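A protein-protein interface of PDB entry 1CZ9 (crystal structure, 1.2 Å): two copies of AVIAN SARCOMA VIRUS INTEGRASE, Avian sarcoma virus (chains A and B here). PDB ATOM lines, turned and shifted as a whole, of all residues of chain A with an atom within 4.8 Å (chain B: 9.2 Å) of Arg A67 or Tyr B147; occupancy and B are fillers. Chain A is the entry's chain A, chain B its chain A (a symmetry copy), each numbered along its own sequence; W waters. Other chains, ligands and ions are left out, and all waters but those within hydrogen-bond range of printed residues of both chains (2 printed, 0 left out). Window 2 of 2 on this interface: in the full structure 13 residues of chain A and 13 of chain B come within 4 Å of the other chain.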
ATOM      1  N   ILE A  62      -6.296  18.350 -12.132  1.00  0.00           N
ATOM      2  CA  ILE A  62      -6.637  17.196 -12.984  1.00  0.00           C
ATOM      3  C   ILE A  62      -5.758  16.024 -12.671  1.00  0.00           C
ATOM      4  O   ILE A  62      -6.220  14.874 -12.654  1.00  0.00           O
ATOM      5  CB  ILE A  62      -6.543  17.630 -14.474  1.00  0.00           C
ATOM      6  CG1 ILE A  62      -7.666  18.609 -14.827  1.00  0.00           C
ATOM      7  CG2 ILE A  62      -6.569  16.426 -15.412  1.00  0.00           C
ATOM      8  CD1 ILE A  62      -7.493  19.277 -16.188  1.00  0.00           C
ATOM      9  N   ALA A  63      -4.450  16.256 -12.429  1.00  0.00           N
ATOM     10  CA  ALA A  63      -3.519  15.205 -12.056  1.00  0.00           C
ATOM     11  C   ALA A  63      -3.881  14.585 -10.688  1.00  0.00           C
ATOM     12  O   ALA A  63      -3.550  13.423 -10.437  1.00  0.00           O
ATOM     13  CB  ALA A  63      -2.110  15.734 -12.012  1.00  0.00           C
ATOM     14  N   LEU A  65      -7.297  14.723  -9.169  1.00  0.00           N
ATOM     15  CA  LEU A  65      -8.676  14.304  -9.063  1.00  0.00           C
ATOM     16  C   LEU A  65      -9.263  13.622 -10.311  1.00  0.00           C
ATOM     17  O   LEU A  65     -10.310  12.998 -10.263  1.00  0.00           O
ATOM     18  CB  LEU A  65      -9.520  15.557  -8.813  1.00  0.00           C
ATOM     19  CG  LEU A  65      -9.287  16.314  -7.515  1.00  0.00           C
ATOM     20  CD1 LEU A  65     -10.209  17.512  -7.383  1.00  0.00           C
ATOM     21  CD2 LEU A  65      -9.452  15.393  -6.310  1.00  0.00           C
ATOM     22  N   GLY A  66      -8.610  13.816 -11.438  1.00  0.00           N
ATOM     23  CA  GLY A  66      -9.126  13.436 -12.735  1.00  0.00           C
ATOM     24  C   GLY A  66      -9.694  14.629 -13.467  1.00  0.00           C
ATOM     25  O   GLY A  66      -9.766  15.739 -12.945  1.00  0.00           O
ATOM     26  N   ARG A  67     -10.101  14.376 -14.711  1.00  0.00           N
ATOM     27  CA  ARG A  67     -10.656  15.435 -15.546  1.00  0.00           C
ATOM     28  C   ARG A  67     -12.134  15.620 -15.224  1.00  0.00           C
ATOM     29  O   ARG A  67     -12.913  14.657 -15.321  1.00  0.00           O
ATOM     30  CB  ARG A  67     -10.517  15.086 -17.034  1.00  0.00           C
ATOM     31  CG  ARG A  67     -10.889  16.220 -17.943  1.00  0.00           C
ATOM     32  CD  ARG A  67     -10.948  16.008 -19.425  1.00  0.00           C
ATOM     33  NE  ARG A  67     -10.100  15.018 -20.029  1.00  0.00           N
ATOM     34  CZ  ARG A  67      -9.575  14.979 -21.262  1.00  0.00           C
ATOM     35  NH1 ARG A  67      -9.742  15.907 -22.207  1.00  0.00           N
ATOM     36  NH2 ARG A  67      -8.820  13.934 -21.582  1.00  0.00           N
ATOM     37  N   PRO A  68     -12.545  16.819 -14.831  1.00  0.00           N
ATOM     38  CA  PRO A  68     -13.970  17.066 -14.484  1.00  0.00           C
ATOM     39  C   PRO A  68     -14.797  17.290 -15.731  1.00  0.00           C
ATOM     40  O   PRO A  68     -14.245  17.633 -16.784  1.00  0.00           O
ATOM     41  CB  PRO A  68     -13.881  18.362 -13.652  1.00  0.00           C
ATOM     42  CG  PRO A  68     -12.743  19.081 -14.331  1.00  0.00           C
ATOM     43  CD  PRO A  68     -11.723  18.020 -14.669  1.00  0.00           C
ATOM     44  N   LYS A  69     -16.098  17.127 -15.602  1.00  0.00           N
ATOM     45  CA  LYS A  69     -17.022  17.488 -16.666  1.00  0.00           C
ATOM     46  C   LYS A  69     -17.252  19.006 -16.764  1.00  0.00           C
ATOM     47  O   LYS A  69     -17.448  19.552 -17.868  1.00  0.00           O
ATOM     48  CB  LYS A  69     -18.354  16.794 -16.459  1.00  0.00           C
ATOM     49  CG  LYS A  69     -18.243  15.265 -16.488  1.00  0.00           C
ATOM     50  CD  LYS A  69     -17.593  14.742 -17.742  1.00  0.00           C
ATOM     51  CE  LYS A  69     -17.908  13.263 -17.970  1.00  0.00           C
ATOM     52  NZ  LYS A  69     -17.755  12.959 -19.420  1.00  0.00           N
ATOM     53  N   TRP A  91      -9.299  21.178 -23.145  1.00  0.00           N
ATOM     54  CA  TRP A  91      -9.484  20.069 -22.235  1.00  0.00           C
ATOM     55  C   TRP A  91     -10.894  19.442 -22.318  1.00  0.00           C
ATOM     56  O   TRP A  91     -11.133  18.391 -21.746  1.00  0.00           O
ATOM     57  CB  TRP A  91      -9.210  20.504 -20.794  1.00  0.00           C
ATOM     58  CG  TRP A  91      -7.765  20.369 -20.401  1.00  0.00           C
ATOM     59  CD1 TRP A  91      -6.781  21.304 -20.342  1.00  0.00           C
ATOM     60  CD2 TRP A  91      -7.163  19.138 -19.995  1.00  0.00           C
ATOM     61  NE1 TRP A  91      -5.604  20.775 -19.948  1.00  0.00           N
ATOM     62  CE2 TRP A  91      -5.811  19.447 -19.715  1.00  0.00           C
ATOM     63  CE3 TRP A  91      -7.605  17.837 -19.828  1.00  0.00           C
ATOM     64  CZ2 TRP A  91      -4.891  18.461 -19.268  1.00  0.00           C
ATOM     65  CZ3 TRP A  91      -6.688  16.887 -19.396  1.00  0.00           C
ATOM     66  CH2 TRP A  91      -5.366  17.201 -19.132  1.00  0.00           C
ATOM     67  N   GLY A  92     -11.820  20.038 -23.055  1.00  0.00           N
ATOM     68  CA  GLY A  92     -13.189  19.560 -23.081  1.00  0.00           C
ATOM     69  C   GLY A  92     -13.956  19.694 -21.782  1.00  0.00           C
ATOM     70  O   GLY A  92     -14.787  18.846 -21.480  1.00  0.00           O
ATOM     71  N   ILE A  93     -13.672  20.720 -21.012  1.00  0.00           N
ATOM     72  CA  ILE A  93     -14.292  20.956 -19.719  1.00  0.00           C
ATOM     73  C   ILE A  93     -15.282  22.101 -19.837  1.00  0.00           C
ATOM     74  O   ILE A  93     -14.873  23.196 -20.266  1.00  0.00           O
ATOM     75  CB  ILE A  93     -13.203  21.237 -18.609  1.00  0.00           C
ATOM     76  CG1 ILE A  93     -12.224  20.110 -18.433  1.00  0.00           C
ATOM     77  CG2 ILE A  93     -13.872  21.656 -17.305  1.00  0.00           C
ATOM     78  CD1 ILE A  93     -10.973  20.439 -17.649  1.00  0.00           C
ATOM     79  N   ALA B  40      -1.064   3.703  -9.313  1.00  0.00           N
ATOM     80  CA  ALA B  40      -1.088   5.171  -9.448  1.00  0.00           C
ATOM     81  C   ALA B  40       0.312   5.733  -9.271  1.00  0.00           C
ATOM     82  O   ALA B  40       1.061   5.261  -8.418  1.00  0.00           O
ATOM     83  CB  ALA B  40      -2.005   5.824  -8.394  1.00  0.00           C
ATOM     84  N   ILE B  41       0.615   6.742 -10.026  1.00  0.00           N
ATOM     85  CA  ILE B  41       1.921   7.412  -9.958  1.00  0.00           C
ATOM     86  C   ILE B  41       1.762   8.860  -9.501  1.00  0.00           C
ATOM     87  O   ILE B  41       0.768   9.553  -9.849  1.00  0.00           O
ATOM     88  CB  ILE B  41       2.520   7.332 -11.377  1.00  0.00           C
ATOM     89  CG1 ILE B  41       2.880   5.883 -11.745  1.00  0.00           C
ATOM     90  CG2 ILE B  41       3.662   8.241 -11.673  1.00  0.00           C
ATOM     91  CD1 ILE B  41       3.025   5.631 -13.260  1.00  0.00           C
ATOM     92  N   VAL B  42       2.747   9.319  -8.730  1.00  0.00           N
ATOM     93  CA  VAL B  42       2.956  10.729  -8.430  1.00  0.00           C
ATOM     94  C   VAL B  42       4.358  11.089  -8.883  1.00  0.00           C
ATOM     95  O   VAL B  42       5.299  10.364  -8.589  1.00  0.00           O
ATOM     96  CB  VAL B  42       2.787  11.056  -6.951  1.00  0.00           C
ATOM     97  CG1 VAL B  42       3.079  12.508  -6.673  1.00  0.00           C
ATOM     98  CG2 VAL B  42       1.362  10.698  -6.508  1.00  0.00           C
ATOM     99  N   VAL B  43       4.490  12.217  -9.605  1.00  0.00           N
ATOM    100  CA  VAL B  43       5.825  12.661 -10.052  1.00  0.00           C
ATOM    101  C   VAL B  43       5.948  14.152  -9.781  1.00  0.00           C
ATOM    102  O   VAL B  43       5.001  14.901 -10.024  1.00  0.00           O
ATOM    103  CB  VAL B  43       6.041  12.335 -11.526  1.00  0.00           C
ATOM    104  CG1 VAL B  43       4.932  12.851 -12.427  1.00  0.00           C
ATOM    105  CG2 VAL B  43       7.386  12.820 -12.020  1.00  0.00           C
ATOM    106  N   LEU B 116       6.571   6.896 -17.772  1.00  0.00           N
ATOM    107  CA  LEU B 116       6.572   8.374 -17.673  1.00  0.00           C
ATOM    108  C   LEU B 116       7.430   8.988 -18.731  1.00  0.00           C
ATOM    109  O   LEU B 116       7.077   9.987 -19.373  1.00  0.00           O
ATOM    110  CB  LEU B 116       7.052   8.647 -16.236  1.00  0.00           C
ATOM    111  CG  LEU B 116       7.119  10.128 -15.933  1.00  0.00           C
ATOM    112  CD1 LEU B 116       5.732  10.780 -16.059  1.00  0.00           C
ATOM    113  CD2 LEU B 116       7.673  10.360 -14.513  1.00  0.00           C
ATOM    114  N   LYS B 119       5.814   8.812 -22.089  1.00  0.00           N
ATOM    115  CA  LYS B 119       4.680   9.723 -22.168  1.00  0.00           C
ATOM    116  C   LYS B 119       5.135  11.174 -22.325  1.00  0.00           C
ATOM    117  O   LYS B 119       4.596  11.958 -23.127  1.00  0.00           O
ATOM    118  CB  LYS B 119       3.762   9.555 -20.993  1.00  0.00           C
ATOM    119  CG  LYS B 119       2.500  10.377 -21.054  1.00  0.00           C
ATOM    120  CD  LYS B 119       1.555  10.028 -22.179  1.00  0.00           C
ATOM    121  CE  LYS B 119       0.862   8.711 -22.059  1.00  0.00           C
ATOM    122  NZ  LYS B 119      -0.059   8.525 -23.232  1.00  0.00           N
ATOM    123  N   LEU B 123       4.178  13.504 -25.519  1.00  0.00           N
ATOM    124  CA  LEU B 123       3.469  14.796 -25.344  1.00  0.00           C
ATOM    125  C   LEU B 123       4.311  15.954 -25.872  1.00  0.00           C
ATOM    126  O   LEU B 123       3.829  16.840 -26.561  1.00  0.00           O
ATOM    127  CB  LEU B 123       3.095  14.998 -23.890  1.00  0.00           C
ATOM    128  CG  LEU B 123       2.094  14.041 -23.289  1.00  0.00           C
ATOM    129  CD1 LEU B 123       1.879  14.361 -21.821  1.00  0.00           C
ATOM    130  CD2 LEU B 123       0.760  14.018 -24.041  1.00  0.00           C
ATOM    131  N   GLY B 139       5.543  22.348 -16.253  1.00  0.00           N
ATOM    132  CA  GLY B 139       4.676  21.900 -15.162  1.00  0.00           C
ATOM    133  C   GLY B 139       3.398  21.309 -15.656  1.00  0.00           C
ATOM    134  O   GLY B 139       2.957  20.241 -15.191  1.00  0.00           O
ATOM    135  N   GLU B 140       2.758  21.962 -16.630  1.00  0.00           N
ATOM    136  CA  GLU B 140       1.496  21.415 -17.128  1.00  0.00           C
ATOM    137  C   GLU B 140       1.717  20.138 -17.913  1.00  0.00           C
ATOM    138  O   GLU B 140       0.893  19.228 -17.885  1.00  0.00           O
ATOM    139  CB  GLU B 140       0.707  22.413 -17.995  1.00  0.00           C
ATOM    140  CG  GLU B 140       0.131  23.573 -17.177  1.00  0.00           C
ATOM    141  CD  GLU B 140      -0.883  24.391 -17.929  1.00  0.00           C
ATOM    142  OE1 GLU B 140      -1.608  23.861 -18.817  1.00  0.00           O
ATOM    143  OE2 GLU B 140      -1.006  25.584 -17.612  1.00  0.00           O
ATOM    144  N   LEU B 141       2.844  20.043 -18.679  1.00  0.00           N
ATOM    145  CA  LEU B 141       3.091  18.832 -19.445  1.00  0.00           C
ATOM    146  C   LEU B 141       3.300  17.654 -18.498  1.00  0.00           C
ATOM    147  O   LEU B 141       2.781  16.550 -18.716  1.00  0.00           O
ATOM    148  CB  LEU B 141       4.243  19.039 -20.435  1.00  0.00           C
ATOM    149  CG  LEU B 141       4.439  17.948 -21.460  1.00  0.00           C
ATOM    150  CD1 LEU B 141       5.046  18.539 -22.727  1.00  0.00           C
ATOM    151  CD2 LEU B 141       5.232  16.784 -20.933  1.00  0.00           C
ATOM    152  N   LEU B 142       4.085  17.843 -17.432  1.00  0.00           N
ATOM    153  CA  LEU B 142       4.299  16.797 -16.450  1.00  0.00           C
ATOM    154  C   LEU B 142       2.992  16.379 -15.782  1.00  0.00           C
ATOM    155  O   LEU B 142       2.723  15.184 -15.616  1.00  0.00           O
ATOM    156  CB  LEU B 142       5.280  17.267 -15.385  1.00  0.00           C
ATOM    157  CG  LEU B 142       5.734  16.188 -14.421  1.00  0.00           C
ATOM    158  CD1 LEU B 142       6.482  15.052 -15.156  1.00  0.00           C
ATOM    159  CD2 LEU B 142       6.600  16.800 -13.332  1.00  0.00           C
ATOM    160  N   ALA B 143       2.150  17.359 -15.446  1.00  0.00           N
ATOM    161  CA  ALA B 143       0.840  17.039 -14.849  1.00  0.00           C
ATOM    162  C   ALA B 143      -0.033  16.272 -15.837  1.00  0.00           C
ATOM    163  O   ALA B 143      -0.821  15.409 -15.402  1.00  0.00           O
ATOM    164  CB  ALA B 143       0.203  18.333 -14.381  1.00  0.00           C
ATOM    165  N   LYS B 144       0.040  16.605 -17.111  1.00  0.00           N
ATOM    166  CA  LYS B 144      -0.739  15.907 -18.134  1.00  0.00           C
ATOM    167  C   LYS B 144      -0.268  14.431 -18.231  1.00  0.00           C
ATOM    168  O   LYS B 144      -1.064  13.523 -18.355  1.00  0.00           O
ATOM    169  CB  LYS B 144      -0.635  16.595 -19.497  1.00  0.00           C
ATOM    170  CG  LYS B 144      -1.420  15.915 -20.587  1.00  0.00           C
ATOM    171  CD  LYS B 144      -1.370  16.596 -21.931  1.00  0.00           C
ATOM    172  CE  LYS B 144      -1.964  17.929 -22.126  1.00  0.00           C
ATOM    173  NZ  LYS B 144      -1.586  18.532 -23.480  1.00  0.00           N
ATOM    174  N   ALA B 145       1.073  14.253 -18.202  1.00  0.00           N
ATOM    175  CA  ALA B 145       1.619  12.896 -18.276  1.00  0.00           C
ATOM    176  C   ALA B 145       1.123  12.072 -17.087  1.00  0.00           C
ATOM    177  O   ALA B 145       0.723  10.922 -17.239  1.00  0.00           O
ATOM    178  CB  ALA B 145       3.135  12.923 -18.310  1.00  0.00           C
ATOM    179  N   MET B 146       1.160  12.676 -15.897  1.00  0.00           N
ATOM    180  CA  MET B 146       0.659  11.984 -14.698  1.00  0.00           C
ATOM    181  C   MET B 146      -0.810  11.632 -14.836  1.00  0.00           C
ATOM    182  O   MET B 146      -1.240  10.491 -14.571  1.00  0.00           O
ATOM    183  CB  MET B 146       0.952  12.854 -13.474  1.00  0.00           C
ATOM    184  CG  MET B 146       0.475  12.269 -12.176  1.00  0.00           C
ATOM    185  SD  MET B 146       1.026  13.296 -10.806  1.00  0.00           S
ATOM    186  CE  MET B 146      -0.171  12.823  -9.541  1.00  0.00           C
ATOM    187  N   TYR B 147      -1.638  12.601 -15.260  1.00  0.00           N
ATOM    188  CA  TYR B 147      -3.042  12.343 -15.529  1.00  0.00           C
ATOM    189  C   TYR B 147      -3.205  11.196 -16.492  1.00  0.00           C
ATOM    190  O   TYR B 147      -4.023  10.282 -16.270  1.00  0.00           O
ATOM    191  CB  TYR B 147      -3.693  13.633 -16.079  1.00  0.00           C
ATOM    192  CG  TYR B 147      -5.007  13.346 -16.761  1.00  0.00           C
ATOM    193  CD1 TYR B 147      -6.164  13.006 -16.069  1.00  0.00           C
ATOM    194  CD2 TYR B 147      -5.092  13.384 -18.147  1.00  0.00           C
ATOM    195  CE1 TYR B 147      -7.352  12.730 -16.761  1.00  0.00           C
ATOM    196  CE2 TYR B 147      -6.240  13.110 -18.863  1.00  0.00           C
ATOM    197  CZ  TYR B 147      -7.369  12.785 -18.131  1.00  0.00           C
ATOM    198  OH  TYR B 147      -8.538  12.525 -18.788  1.00  0.00           O
ATOM    199  N   ALA B 148      -2.485  11.209 -17.620  1.00  0.00           N
ATOM    200  CA  ALA B 148      -2.680  10.218 -18.681  1.00  0.00           C
ATOM    201  C   ALA B 148      -2.352   8.840 -18.157  1.00  0.00           C
ATOM    202  O   ALA B 148      -3.035   7.849 -18.477  1.00  0.00           O
ATOM    203  CB  ALA B 148      -1.827  10.616 -19.862  1.00  0.00           C
ATOM    204  N   LEU B 149      -1.282   8.714 -17.381  1.00  0.00           N
ATOM    205  CA  LEU B 149      -0.876   7.390 -16.890  1.00  0.00           C
ATOM    206  C   LEU B 149      -1.799   6.877 -15.814  1.00  0.00           C
ATOM    207  O   LEU B 149      -1.959   5.650 -15.708  1.00  0.00           O
ATOM    208  CB  LEU B 149       0.575   7.458 -16.450  1.00  0.00           C
ATOM    209  CG  LEU B 149       1.603   7.687 -17.595  1.00  0.00           C
ATOM    210  CD1 LEU B 149       2.978   7.914 -17.014  1.00  0.00           C
ATOM    211  CD2 LEU B 149       1.600   6.508 -18.543  1.00  0.00           C
ATOM    212  N   ASN B 150      -2.441   7.783 -15.061  1.00  0.00           N
ATOM    213  CA  ASN B 150      -3.265   7.299 -13.963  1.00  0.00           C
ATOM    214  C   ASN B 150      -4.700   7.011 -14.444  1.00  0.00           C
ATOM    215  O   ASN B 150      -5.520   6.451 -13.743  1.00  0.00           O
ATOM    216  CB  ASN B 150      -3.242   8.316 -12.829  1.00  0.00           C
ATOM    217  CG  ASN B 150      -1.931   8.246 -12.081  1.00  0.00           C
ATOM    218  OD1 ASN B 150      -1.192   7.254 -12.157  1.00  0.00           O
ATOM    219  ND2 ASN B 150      -1.599   9.288 -11.391  1.00  0.00           N
HETATM  220  O   HOH W   1      -3.402  11.483 -12.137  1.00  0.00           O
HETATM  221  O   HOH W   2      -2.761  21.392 -19.316  1.00  0.00           O
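Of the 19 printed residues of chain B, 3 touch a printed residue of chain A.
Hydrophobic or aromatic side chains of chain B that line the printed part of chain A: Met B146 and Tyr B147.
Printed residues of chain A that touch a printed residue of chain B: Ile A62, Ala A63, Arg A67 and Trp A91.
Hydrophobic or aromatic side chains of chain A that line the printed part of chain B: Ile A62, Ala A63 and Trp A91.
Among the printed residues, 5 pairs touch across the chains.
Among the printed residues, no Asp or Glu carboxylate lies within 4 Å of a Lys or Arg side-chain nitrogen of the other chain.
NH1 of Arg A67 is in hydrogen-bond range of O of Trp A91 (2.9 Å).
The backbone carbonyl oxygen (O) of Met B146 is in hydrogen-bond range of the side-chain amide nitrogen (ND2) of Asn B150.
Of the printed residues of chain B, Arg A67 touches Tyr B147.
Printed residues of chain A within 4 Å of Tyr B147: Ile A62 (3.5 Å), Arg A67 (3.1 Å) and Trp A91 (3.8 Å).
No residue of chain B comes within 4 Å of Pro A68.
Of the printed residues of chain B, Trp A91 touches Tyr B147.
Printed residues of chain B within 4 Å of Ala A63: Ala B143 and Met B146.
Of the printed residues of chain A, Ala B143 touches Ala A63.
Printed residues of chain A within 4 Å of Met B146: Ala A63.
Glu B140 touches none of the printed residues of chain A.
Ala B145 touches none of the printed residues of chain A.
The nearest printed residue of chain A that does not touch Tyr B147 is Ala A63 (4.3 Å).
The nearest printed residue of chain A that does not touch Ala B143 is Ile A62 (5.7 Å).
NH2 of Arg A67 lies within hydrogen-bond range of OH of Tyr B147 (3.1 Å).
Among the printed residues, merely in contact across the chains: Ile A62 with Tyr B147, Ala A63 with Ala B143, Ala A63 with Met B146 and Trp A91 with Tyr B147.
No position is printed for both chains.
Of the 5 pairs that touch across the chains among the printed residues, none has its exchanged pair printed and touching as well.
Water W1 lies within hydrogen-bond range of the backbone carbonyl oxygen (O) of Ala A63 (2.6 Å), the side-chain amide nitrogen (ND2) of Asn B150 (2.9 Å) and the backbone carbonyl oxygen (O) of Met B146 (3.4 Å).
Water W2 lies within hydrogen-bond range of OE1 of Glu B140 (2.8 Å) and NE1 of Trp A91 (3.0 Å).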
